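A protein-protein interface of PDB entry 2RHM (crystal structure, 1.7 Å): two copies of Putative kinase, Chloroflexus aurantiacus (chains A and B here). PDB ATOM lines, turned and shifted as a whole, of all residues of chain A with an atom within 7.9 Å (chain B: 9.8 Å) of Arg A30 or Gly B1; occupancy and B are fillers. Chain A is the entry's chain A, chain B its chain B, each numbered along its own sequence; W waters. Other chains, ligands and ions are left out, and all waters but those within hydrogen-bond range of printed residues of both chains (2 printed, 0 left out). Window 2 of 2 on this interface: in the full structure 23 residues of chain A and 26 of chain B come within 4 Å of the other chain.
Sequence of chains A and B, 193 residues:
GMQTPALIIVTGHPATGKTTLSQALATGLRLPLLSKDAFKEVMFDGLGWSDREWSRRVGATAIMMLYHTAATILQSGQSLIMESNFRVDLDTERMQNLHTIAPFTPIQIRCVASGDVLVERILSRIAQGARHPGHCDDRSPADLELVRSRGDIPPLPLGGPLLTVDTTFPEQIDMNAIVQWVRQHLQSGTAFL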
ATOM      1  N   GLN A  23      -9.772  11.901   9.010  1.00  0.00           N
ATOM      2  CA  GLN A  23      -9.572  13.210   8.409  1.00  0.00           C
ATOM      3  C   GLN A  23      -9.118  14.232   9.452  1.00  0.00           C
ATOM      4  O   GLN A  23      -8.263  15.078   9.163  1.00  0.00           O
ATOM      5  CB  GLN A  23     -10.842  13.652   7.675  1.00  0.00           C
ATOM      6  CG  GLN A  23     -11.092  12.837   6.398  1.00  0.00           C
ATOM      7  CD  GLN A  23     -12.480  13.033   5.797  1.00  0.00           C
ATOM      8  OE1 GLN A  23     -13.315  13.766   6.334  1.00  0.00           O
ATOM      9  NE2 GLN A  23     -12.744  12.338   4.699  1.00  0.00           N
ATOM     10  N   ALA A  24      -9.673  14.144  10.662  1.00  0.00           N
ATOM     11  CA  ALA A  24      -9.271  15.016  11.761  1.00  0.00           C
ATOM     12  C   ALA A  24      -7.835  14.720  12.171  1.00  0.00           C
ATOM     13  O   ALA A  24      -7.069  15.637  12.473  1.00  0.00           O
ATOM     14  CB  ALA A  24     -10.200  14.842  12.948  1.00  0.00           C
ATOM     15  N   LEU A  25      -7.466  13.441  12.205  1.00  0.00           N
ATOM     16  CA  LEU A  25      -6.080  13.092  12.494  1.00  0.00           C
ATOM     17  C   LEU A  25      -5.139  13.617  11.428  1.00  0.00           C
ATOM     18  O   LEU A  25      -4.050  14.106  11.745  1.00  0.00           O
ATOM     19  CB  LEU A  25      -5.908  11.584  12.611  1.00  0.00           C
ATOM     20  CG  LEU A  25      -6.461  10.955  13.884  1.00  0.00           C
ATOM     21  CD1 LEU A  25      -6.297   9.463  13.800  1.00  0.00           C
ATOM     22  CD2 LEU A  25      -5.786  11.495  15.147  1.00  0.00           C
ATOM     23  N   ALA A  26      -5.543  13.521  10.166  1.00  0.00           N
ATOM     24  CA  ALA A  26      -4.644  13.911   9.067  1.00  0.00           C
ATOM     25  C   ALA A  26      -4.393  15.396   9.134  1.00  0.00           C
ATOM     26  O   ALA A  26      -3.257  15.849   9.096  1.00  0.00           O
ATOM     27  CB  ALA A  26      -5.221  13.516   7.717  1.00  0.00           C
ATOM     28  N   THR A  27      -5.475  16.145   9.284  1.00  0.00           N
ATOM     29  CA  THR A  27      -5.392  17.586   9.342  1.00  0.00           C
ATOM     30  C   THR A  27      -4.736  18.060  10.653  1.00  0.00           C
ATOM     31  O   THR A  27      -3.957  19.017  10.651  1.00  0.00           O
ATOM     32  CB  THR A  27      -6.790  18.200   9.125  1.00  0.00           C
ATOM     33  OG1 THR A  27      -6.657  19.573   8.765  1.00  0.00           O
ATOM     34  CG2 THR A  27      -7.657  18.072  10.355  1.00  0.00           C
ATOM     35  N   GLY A  28      -5.027  17.367  11.755  1.00  0.00           N
ATOM     36  CA  GLY A  28      -4.486  17.709  13.062  1.00  0.00           C
ATOM     37  C   GLY A  28      -2.999  17.434  13.227  1.00  0.00           C
ATOM     38  O   GLY A  28      -2.298  18.196  13.892  1.00  0.00           O
ATOM     39  N   LEU A  29      -2.524  16.341  12.637  1.00  0.00           N
ATOM     40  CA  LEU A  29      -1.118  15.948  12.709  1.00  0.00           C
ATOM     41  C   LEU A  29      -0.343  16.365  11.464  1.00  0.00           C
ATOM     42  O   LEU A  29       0.871  16.251  11.437  1.00  0.00           O
ATOM     43  CB  LEU A  29      -0.994  14.431  12.846  1.00  0.00           C
ATOM     44  CG  LEU A  29      -1.649  13.794  14.074  1.00  0.00           C
ATOM     45  CD1 LEU A  29      -1.648  12.284  13.919  1.00  0.00           C
ATOM     46  CD2 LEU A  29      -0.908  14.231  15.312  1.00  0.00           C
ATOM     47  N   ARG A  30      -1.054  16.828  10.442  1.00  0.00           N
ATOM     48  CA  ARG A  30      -0.456  17.190   9.159  1.00  0.00           C
ATOM     49  C   ARG A  30       0.266  15.977   8.548  1.00  0.00           C
ATOM     50  O   ARG A  30       1.465  16.027   8.271  1.00  0.00           O
ATOM     51  CB  ARG A  30       0.494  18.383   9.338  1.00  0.00           C
ATOM     52  CG  ARG A  30       0.658  19.246   8.091  1.00  0.00           C
ATOM     53  CD  ARG A  30       1.924  20.089   8.138  1.00  0.00           C
ATOM     54  NE  ARG A  30       2.114  20.860   6.905  1.00  0.00           N
ATOM     55  CZ  ARG A  30       3.289  21.282   6.436  1.00  0.00           C
ATOM     56  NH1 ARG A  30       4.425  21.005   7.067  1.00  0.00           N
ATOM     57  NH2 ARG A  30       3.335  21.976   5.303  1.00  0.00           N
ATOM     58  N   LEU A  31      -0.475  14.881   8.369  1.00  0.00           N
ATOM     59  CA  LEU A  31       0.058  13.667   7.776  1.00  0.00           C
ATOM     60  C   LEU A  31      -0.791  13.291   6.569  1.00  0.00           C
ATOM     61  O   LEU A  31      -1.967  13.667   6.506  1.00  0.00           O
ATOM     62  CB  LEU A  31       0.050  12.503   8.778  1.00  0.00           C
ATOM     63  CG  LEU A  31       1.005  12.578   9.971  1.00  0.00           C
ATOM     64  CD1 LEU A  31       0.928  11.314  10.774  1.00  0.00           C
ATOM     65  CD2 LEU A  31       2.427  12.825   9.506  1.00  0.00           C
ATOM     66  N   PRO A  32      -0.206  12.529   5.623  1.00  0.00           N
ATOM     67  CA  PRO A  32      -0.973  12.021   4.500  1.00  0.00           C
ATOM     68  C   PRO A  32      -2.012  11.011   4.956  1.00  0.00           C
ATOM     69  O   PRO A  32      -1.816  10.297   5.951  1.00  0.00           O
ATOM     70  CB  PRO A  32       0.089  11.333   3.619  1.00  0.00           C
ATOM     71  CG  PRO A  32       1.401  11.836   4.110  1.00  0.00           C
ATOM     72  CD  PRO A  32       1.189  12.061   5.565  1.00  0.00           C
ATOM     73  N   LEU A  33      -3.124  10.965   4.237  1.00  0.00           N
ATOM     74  CA  LEU A  33      -4.210  10.041   4.532  1.00  0.00           C
ATOM     75  C   LEU A  33      -4.551   9.218   3.324  1.00  0.00           C
ATOM     76  O   LEU A  33      -4.872   9.766   2.272  1.00  0.00           O
ATOM     77  CB  LEU A  33      -5.446  10.816   4.968  1.00  0.00           C
ATOM     78  CG  LEU A  33      -6.771  10.076   5.162  1.00  0.00           C
ATOM     79  CD1 LEU A  33      -6.701   9.073   6.275  1.00  0.00           C
ATOM     80  CD2 LEU A  33      -7.852  11.092   5.451  1.00  0.00           C
ATOM     81  N   GLN A  78       8.421   9.200   5.895  1.00  0.00           N
ATOM     82  CA  GLN A  78       7.256  10.010   6.232  1.00  0.00           C
ATOM     83  C   GLN A  78       6.198   9.126   6.893  1.00  0.00           C
ATOM     84  O   GLN A  78       5.944   8.009   6.442  1.00  0.00           O
ATOM     85  CB  GLN A  78       6.697  10.687   4.960  1.00  0.00           C
ATOM     86  CG  GLN A  78       5.332  11.409   5.111  1.00  0.00           C
ATOM     87  CD  GLN A  78       5.412  12.728   5.880  1.00  0.00           C
ATOM     88  OE1 GLN A  78       6.324  13.524   5.679  1.00  0.00           O
ATOM     89  NE2 GLN A  78       4.444  12.962   6.752  1.00  0.00           N
ATOM     90  N   SER A  79       5.603   9.619   7.972  1.00  0.00           N
ATOM     91  CA  SER A  79       4.531   8.897   8.642  1.00  0.00           C
ATOM     92  C   SER A  79       3.230   9.118   7.887  1.00  0.00           C
ATOM     93  O   SER A  79       3.102  10.069   7.100  1.00  0.00           O
ATOM     94  CB  SER A  79       4.382   9.353  10.102  1.00  0.00           C
ATOM     95  OG  SER A  79       5.533   9.027  10.872  1.00  0.00           O
ATOM     96  N   LEU A  80       2.265   8.233   8.101  1.00  0.00           N
ATOM     97  CA  LEU A  80       1.000   8.352   7.406  1.00  0.00           C
ATOM     98  C   LEU A  80      -0.135   7.672   8.145  1.00  0.00           C
ATOM     99  O   LEU A  80       0.086   6.923   9.106  1.00  0.00           O
ATOM    100  CB  LEU A  80       1.129   7.799   5.975  1.00  0.00           C
ATOM    101  CG  LEU A  80       1.234   6.286   5.825  1.00  0.00           C
ATOM    102  CD1 LEU A  80      -0.083   5.743   5.393  1.00  0.00           C
ATOM    103  CD2 LEU A  80       2.285   5.903   4.798  1.00  0.00           C
ATOM    104  N   ILE A  81      -1.347   7.979   7.697  1.00  0.00           N
ATOM    105  CA  ILE A  81      -2.577   7.397   8.219  1.00  0.00           C
ATOM    106  C   ILE A  81      -3.221   6.532   7.135  1.00  0.00           C
ATOM    107  O   ILE A  81      -3.343   6.951   5.978  1.00  0.00           O
ATOM    108  CB  ILE A  81      -3.575   8.492   8.633  1.00  0.00           C
ATOM    109  CG1 ILE A  81      -2.965   9.421   9.686  1.00  0.00           C
ATOM    110  CG2 ILE A  81      -4.862   7.876   9.172  1.00  0.00           C
ATOM    111  CD1 ILE A  81      -3.519  10.815   9.617  1.00  0.00           C
ATOM    112  N   VAL A 179      -6.198  13.337  18.981  1.00  0.00           N
ATOM    113  CA  VAL A 179      -5.005  13.799  18.273  1.00  0.00           C
ATOM    114  C   VAL A 179      -3.796  13.767  19.192  1.00  0.00           C
ATOM    115  O   VAL A 179      -2.733  13.271  18.813  1.00  0.00           O
ATOM    116  CB  VAL A 179      -5.164  15.236  17.715  1.00  0.00           C
ATOM    117  CG1 VAL A 179      -3.820  15.782  17.210  1.00  0.00           C
ATOM    118  CG2 VAL A 179      -6.201  15.264  16.608  1.00  0.00           C
ATOM    119  N   ARG A 183      -0.318  11.907  18.981  1.00  0.00           N
ATOM    120  CA  ARG A 183       0.867  12.764  18.929  1.00  0.00           C
ATOM    121  C   ARG A 183       1.848  12.472  20.067  1.00  0.00           C
ATOM    122  O   ARG A 183       3.063  12.575  19.878  1.00  0.00           O
ATOM    123  CB  ARG A 183       0.476  14.247  18.910  1.00  0.00           C
ATOM    124  CG  ARG A 183       1.666  15.195  18.956  1.00  0.00           C
ATOM    125  CD  ARG A 183       1.307  16.616  18.530  1.00  0.00           C
ATOM    126  NE  ARG A 183       1.197  16.755  17.077  1.00  0.00           N
ATOM    127  CZ  ARG A 183       2.229  16.822  16.235  1.00  0.00           C
ATOM    128  NH1 ARG A 183       3.480  16.738  16.679  1.00  0.00           N
ATOM    129  NH2 ARG A 183       2.010  16.956  14.933  1.00  0.00           N
ATOM    130  N   GLY B   1       8.168  21.994   9.269  1.00  0.00           N
ATOM    131  CA  GLY B   1       8.221  23.451   8.965  1.00  0.00           C
ATOM    132  C   GLY B   1       7.123  23.918   8.026  1.00  0.00           C
ATOM    133  O   GLY B   1       6.270  23.134   7.613  1.00  0.00           O
ATOM    134  N   MET B   2       7.171  25.198   7.675  1.00  0.00           N
ATOM    135  CA  MET B   2       6.160  25.839   6.847  1.00  0.00           C
ATOM    136  C   MET B   2       6.549  25.904   5.372  1.00  0.00           C
ATOM    137  O   MET B   2       5.817  26.493   4.582  1.00  0.00           O
ATOM    138  CB  MET B   2       5.936  27.279   7.315  1.00  0.00           C
ATOM    139  CG  MET B   2       5.266  27.431   8.660  1.00  0.00           C
ATOM    140  SD  MET B   2       4.974  29.336   9.137  1.00  0.00           S
ATOM    141  CE  MET B   2       4.071  30.029   7.445  1.00  0.00           C
ATOM    142  N   GLN B   3       7.683  25.315   5.006  1.00  0.00           N
ATOM    143  CA  GLN B   3       8.174  25.409   3.626  1.00  0.00           C
ATOM    144  C   GLN B   3       7.169  24.785   2.680  1.00  0.00           C
ATOM    145  O   GLN B   3       6.543  23.773   2.988  1.00  0.00           O
ATOM    146  CB  GLN B   3       9.503  24.660   3.375  1.00  0.00           C
ATOM    147  CG  GLN B   3      10.371  24.387   4.552  1.00  0.00           C
ATOM    148  CD  GLN B   3      10.003  23.094   5.247  1.00  0.00           C
ATOM    149  OE1 GLN B   3       9.281  23.104   6.229  1.00  0.00           O
ATOM    150  NE2 GLN B   3      10.477  21.974   4.719  1.00  0.00           N
ATOM    151  N   THR B   4       7.063  25.362   1.498  1.00  0.00           N
ATOM    152  CA  THR B   4       6.290  24.752   0.429  1.00  0.00           C
ATOM    153  C   THR B   4       7.040  23.497  -0.057  1.00  0.00           C
ATOM    154  O   THR B   4       8.244  23.555  -0.296  1.00  0.00           O
ATOM    155  CB  THR B   4       6.139  25.732  -0.738  1.00  0.00           C
ATOM    156  OG1 THR B   4       5.553  26.960  -0.267  1.00  0.00           O
ATOM    157  CG2 THR B   4       5.280  25.121  -1.865  1.00  0.00           C
ATOM    158  N   PRO B   5       6.343  22.359  -0.177  1.00  0.00           N
ATOM    159  CA  PRO B   5       7.012  21.160  -0.676  1.00  0.00           C
ATOM    160  C   PRO B   5       7.321  21.213  -2.151  1.00  0.00           C
ATOM    161  O   PRO B   5       6.671  21.956  -2.890  1.00  0.00           O
ATOM    162  CB  PRO B   5       5.992  20.063  -0.405  1.00  0.00           C
ATOM    163  CG  PRO B   5       4.703  20.740  -0.456  1.00  0.00           C
ATOM    164  CD  PRO B   5       4.937  22.080   0.167  1.00  0.00           C
ATOM    165  N   ALA B   6       8.308  20.435  -2.581  1.00  0.00           N
ATOM    166  CA  ALA B   6       8.638  20.347  -3.994  1.00  0.00           C
ATOM    167  C   ALA B   6       7.852  19.238  -4.648  1.00  0.00           C
ATOM    168  O   ALA B   6       7.586  18.199  -4.035  1.00  0.00           O
ATOM    169  CB  ALA B   6      10.135  20.099  -4.197  1.00  0.00           C
ATOM    170  N   ALA B  71      -1.945  14.943  -3.710  1.00  0.00           N
ATOM    171  CA  ALA B  71      -2.497  16.044  -2.941  1.00  0.00           C
ATOM    172  C   ALA B  71      -2.328  15.792  -1.459  1.00  0.00           C
ATOM    173  O   ALA B  71      -1.970  16.693  -0.701  1.00  0.00           O
ATOM    174  CB  ALA B  71      -3.953  16.227  -3.274  1.00  0.00           C
ATOM    175  N   THR B  72      -2.602  14.572  -1.016  1.00  0.00           N
ATOM    176  CA  THR B  72      -2.505  14.331   0.422  1.00  0.00           C
ATOM    177  C   THR B  72      -1.045  14.345   0.908  1.00  0.00           C
ATOM    178  O   THR B  72      -0.774  14.739   2.028  1.00  0.00           O
ATOM    179  CB  THR B  72      -3.270  13.062   0.874  1.00  0.00           C
ATOM    180  OG1 THR B  72      -3.362  13.050   2.308  1.00  0.00           O
ATOM    181  CG2 THR B  72      -2.592  11.780   0.369  1.00  0.00           C
ATOM    182  N   ILE B  73      -0.111  13.925   0.058  1.00  0.00           N
ATOM    183  CA  ILE B  73       1.321  13.962   0.408  1.00  0.00           C
ATOM    184  C   ILE B  73       1.805  15.406   0.478  1.00  0.00           C
ATOM    185  O   ILE B  73       2.471  15.818   1.444  1.00  0.00           O
ATOM    186  CB  ILE B  73       2.157  13.153  -0.610  1.00  0.00           C
ATOM    187  CG1 ILE B  73       1.776  11.673  -0.540  1.00  0.00           C
ATOM    188  CG2 ILE B  73       3.637  13.303  -0.346  1.00  0.00           C
ATOM    189  CD1 ILE B  73       2.406  10.840  -1.575  1.00  0.00           C
ATOM    190  N   LEU B  74       1.463  16.181  -0.544  1.00  0.00           N
ATOM    191  CA  LEU B  74       1.842  17.597  -0.581  1.00  0.00           C
ATOM    192  C   LEU B  74       1.231  18.399   0.563  1.00  0.00           C
ATOM    193  O   LEU B  74       1.902  19.281   1.138  1.00  0.00           O
ATOM    194  CB  LEU B  74       1.473  18.216  -1.935  1.00  0.00           C
ATOM    195  CG  LEU B  74       2.295  17.710  -3.131  1.00  0.00           C
ATOM    196  CD1 LEU B  74       1.735  18.231  -4.432  1.00  0.00           C
ATOM    197  CD2 LEU B  74       3.758  18.129  -3.002  1.00  0.00           C
ATOM    198  N   GLN B  75      -0.027  18.092   0.903  1.00  0.00           N
ATOM    199  CA  GLN B  75      -0.717  18.765   2.007  1.00  0.00           C
ATOM    200  C   GLN B  75      -0.035  18.515   3.367  1.00  0.00           C
ATOM    201  O   GLN B  75      -0.135  19.344   4.264  1.00  0.00           O
ATOM    202  CB  GLN B  75      -2.180  18.348   2.042  1.00  0.00           C
ATOM    203  CG  GLN B  75      -3.005  18.986   0.924  1.00  0.00           C
ATOM    204  CD  GLN B  75      -4.386  18.347   0.708  1.00  0.00           C
ATOM    205  OE1 GLN B  75      -4.696  17.283   1.246  1.00  0.00           O
ATOM    206  NE2 GLN B  75      -5.208  19.001  -0.094  1.00  0.00           N
ATOM    207  N   SER B  76       0.673  17.391   3.506  1.00  0.00           N
ATOM    208  CA  SER B  76       1.432  17.081   4.729  1.00  0.00           C
ATOM    209  C   SER B  76       2.794  17.799   4.777  1.00  0.00           C
ATOM    210  O   SER B  76       3.492  17.759   5.790  1.00  0.00           O
ATOM    211  CB  SER B  76       1.657  15.568   4.850  1.00  0.00           C
ATOM    212  OG  SER B  76       2.718  15.144   4.008  1.00  0.00           O
ATOM    213  N   GLY B  77       3.169  18.439   3.673  1.00  0.00           N
ATOM    214  CA  GLY B  77       4.420  19.199   3.576  1.00  0.00           C
ATOM    215  C   GLY B  77       5.593  18.406   3.043  1.00  0.00           C
ATOM    216  O   GLY B  77       6.728  18.881   3.073  1.00  0.00           O
ATOM    217  N   GLN B  78       5.309  17.217   2.510  1.00  0.00           N
ATOM    218  CA  GLN B  78       6.331  16.319   2.014  1.00  0.00           C
ATOM    219  C   GLN B  78       6.439  16.502   0.514  1.00  0.00           C
ATOM    220  O   GLN B  78       5.430  16.664  -0.188  1.00  0.00           O
ATOM    221  CB  GLN B  78       5.982  14.867   2.380  1.00  0.00           C
ATOM    222  CG  GLN B  78       6.796  13.725   1.722  1.00  0.00           C
ATOM    223  CD  GLN B  78       8.276  13.705   2.072  1.00  0.00           C
ATOM    224  OE1 GLN B  78       8.994  14.696   1.911  1.00  0.00           O
ATOM    225  NE2 GLN B  78       8.746  12.553   2.535  1.00  0.00           N
ATOM    226  N   SER B  79       7.679  16.489   0.037  1.00  0.00           N
ATOM    227  CA  SER B  79       7.965  16.558  -1.378  1.00  0.00           C
ATOM    228  C   SER B  79       7.778  15.170  -2.007  1.00  0.00           C
ATOM    229  O   SER B  79       7.778  14.142  -1.314  1.00  0.00           O
ATOM    230  CB  SER B  79       9.384  17.075  -1.603  1.00  0.00           C
ATOM    231  OG  SER B  79       9.566  18.359  -1.018  1.00  0.00           O
ATOM    232  N   ALA B 102      -3.056  22.033  -2.859  1.00  0.00           N
ATOM    233  CA  ALA B 102      -1.843  21.484  -2.288  1.00  0.00           C
ATOM    234  C   ALA B 102      -0.652  22.163  -2.948  1.00  0.00           C
ATOM    235  O   ALA B 102      -0.050  21.595  -3.862  1.00  0.00           O
ATOM    236  CB  ALA B 102      -1.835  19.993  -2.563  1.00  0.00           C
ATOM    237  N   PRO B 103      -0.337  23.399  -2.516  1.00  0.00           N
ATOM    238  CA  PRO B 103       0.753  24.168  -3.101  1.00  0.00           C
ATOM    239  C   PRO B 103       2.099  23.443  -3.128  1.00  0.00           C
ATOM    240  O   PRO B 103       2.471  22.757  -2.184  1.00  0.00           O
ATOM    241  CB  PRO B 103       0.812  25.433  -2.234  1.00  0.00           C
ATOM    242  CG  PRO B 103      -0.043  25.182  -1.085  1.00  0.00           C
ATOM    243  CD  PRO B 103      -1.041  24.172  -1.481  1.00  0.00           C
ATOM    244  N   PHE B 104       2.810  23.612  -4.232  1.00  0.00           N
ATOM    245  CA  PHE B 104       4.076  22.957  -4.460  1.00  0.00           C
ATOM    246  C   PHE B 104       4.927  23.863  -5.310  1.00  0.00           C
ATOM    247  O   PHE B 104       4.423  24.767  -5.972  1.00  0.00           O
ATOM    248  CB  PHE B 104       3.897  21.610  -5.184  1.00  0.00           C
ATOM    249  CG  PHE B 104       3.183  21.717  -6.529  1.00  0.00           C
ATOM    250  CD1 PHE B 104       3.883  22.062  -7.671  1.00  0.00           C
ATOM    251  CD2 PHE B 104       1.831  21.440  -6.648  1.00  0.00           C
ATOM    252  CE1 PHE B 104       3.221  22.205  -8.892  1.00  0.00           C
ATOM    253  CE2 PHE B 104       1.175  21.572  -7.859  1.00  0.00           C
ATOM    254  CZ  PHE B 104       1.863  21.930  -8.980  1.00  0.00           C
HETATM  255  O   HOH W   1      -6.623  12.069   1.754  1.00  0.00           O
HETATM  256  O   HOH W   2       7.558  20.000   6.638  1.00  0.00           O
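The backbone NH (N) of Leu A33 sits at hydrogen-bond distance from the side-chain hydroxyl (OG1) of Thr B72 (2.9 Å). The backbone carbonyl oxygen (O) of Gly B1 lies within hydrogen-bond range of the guanidinium group (NH1) of Arg A30.
Of the 18 printed residues of chain B, 6 touch a printed residue of chain A. Of the 17 printed residues of chain A, 5 touch a printed residue of chain B. Printed residues of chain A that touch a printed residue of chain B: Arg A30, Leu A31, Pro A32, Leu A33 and Gln A78. Among the printed residues, 10 pairs touch across the chains. Among the printed residues, no Asp or Glu carboxylate lies within 4 Å of a Lys or Arg side-chain nitrogen of the other chain.
O of Gln B75 touches NE of Arg A30, at 3.8 Å. Arg A30 touches Ser B76. NH2 of Arg A30 touches CA of Gly B77, 3.4 Å away. CB of Ser B76 touches C of Leu A31, at 3.8 Å. Pro A32 touches Thr B72 (CA to OG1, 3.4 Å). OG of Ser B76 touches CG of Pro A32 (3.6 Å). Ser B76 touches Gln A78. Gln A78 touches Gln B78 (OE1 to CB, 3.6 Å).
Water W1 bridges the backbone carbonyl oxygen (O) of Leu A33 (2.9 Å) and the side-chain hydroxyl (OG1) of Thr B72 (3.5 Å). Water W2 lies within hydrogen-bond range of the guanidinium group (NH1) of Arg A30 (3.3 Å) and the backbone NH (N) of Gly B1 (3.4 Å).
Arg A30 touches just these residues of chain B: Gly B1, Gln B75, Ser B76 and Gly B77. Gly B1 touches just one residue of chain A: Arg A30 (2.9 Å). No residue of chain B comes within 4 Å of Gly A28. Of chain B, only Ser B76 (3.8 Å) comes within 4 Å of Leu A31. Of the printed residues of chain A, Ser B76 touches Arg A30, Leu A31, Pro A32 and Gln A78. Of the printed residues of chain A, Gln B78 touches Gln A78. Printed residues of chain A within 4 Å of Gln B75: Arg A30 (3.8 Å). Of the printed residues of chain B, Leu A33 touches Thr B72 (2.9 Å). Of the printed residues of chain A, Thr B72 touches Pro A32 and Leu A33. Ala A26 touches none of the printed residues of chain B. Pro B103 touches none of the printed residues of chain A.
The backbone carbonyl oxygen of Ile B73 is in hydrogen-bond range of the backbone NH of Gln B78, at 3.3 Å. O of Pro A32 sits at hydrogen-bond distance from N of Ile A81, 2.9 Å away. The backbone carbonyl oxygen (O) of Gly B1 sits close to the side-chain amide oxygen (OE1) of Gln B3 (3.3 Å). O of Ile B73 sits at hydrogen-bond distance from OG of Ser B76, at 2.7 Å. The backbone carbonyl oxygen (O) of Ala A26 lies within hydrogen-bond range of the backbone NH (N) of Leu A31 (3.0 Å). The backbone carbonyl oxygen (O) of Ala B71 sits close to the side-chain amide oxygen (OE1) of Gln B75, at 3.4 Å.
Gln B78 touches its own counterpart, Gln A78. Positions printed for both chains: 78 and 79. Of the 10 pairs that touch across the chains among the printed residues, 1 has its exchanged pair printed and touching as well.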
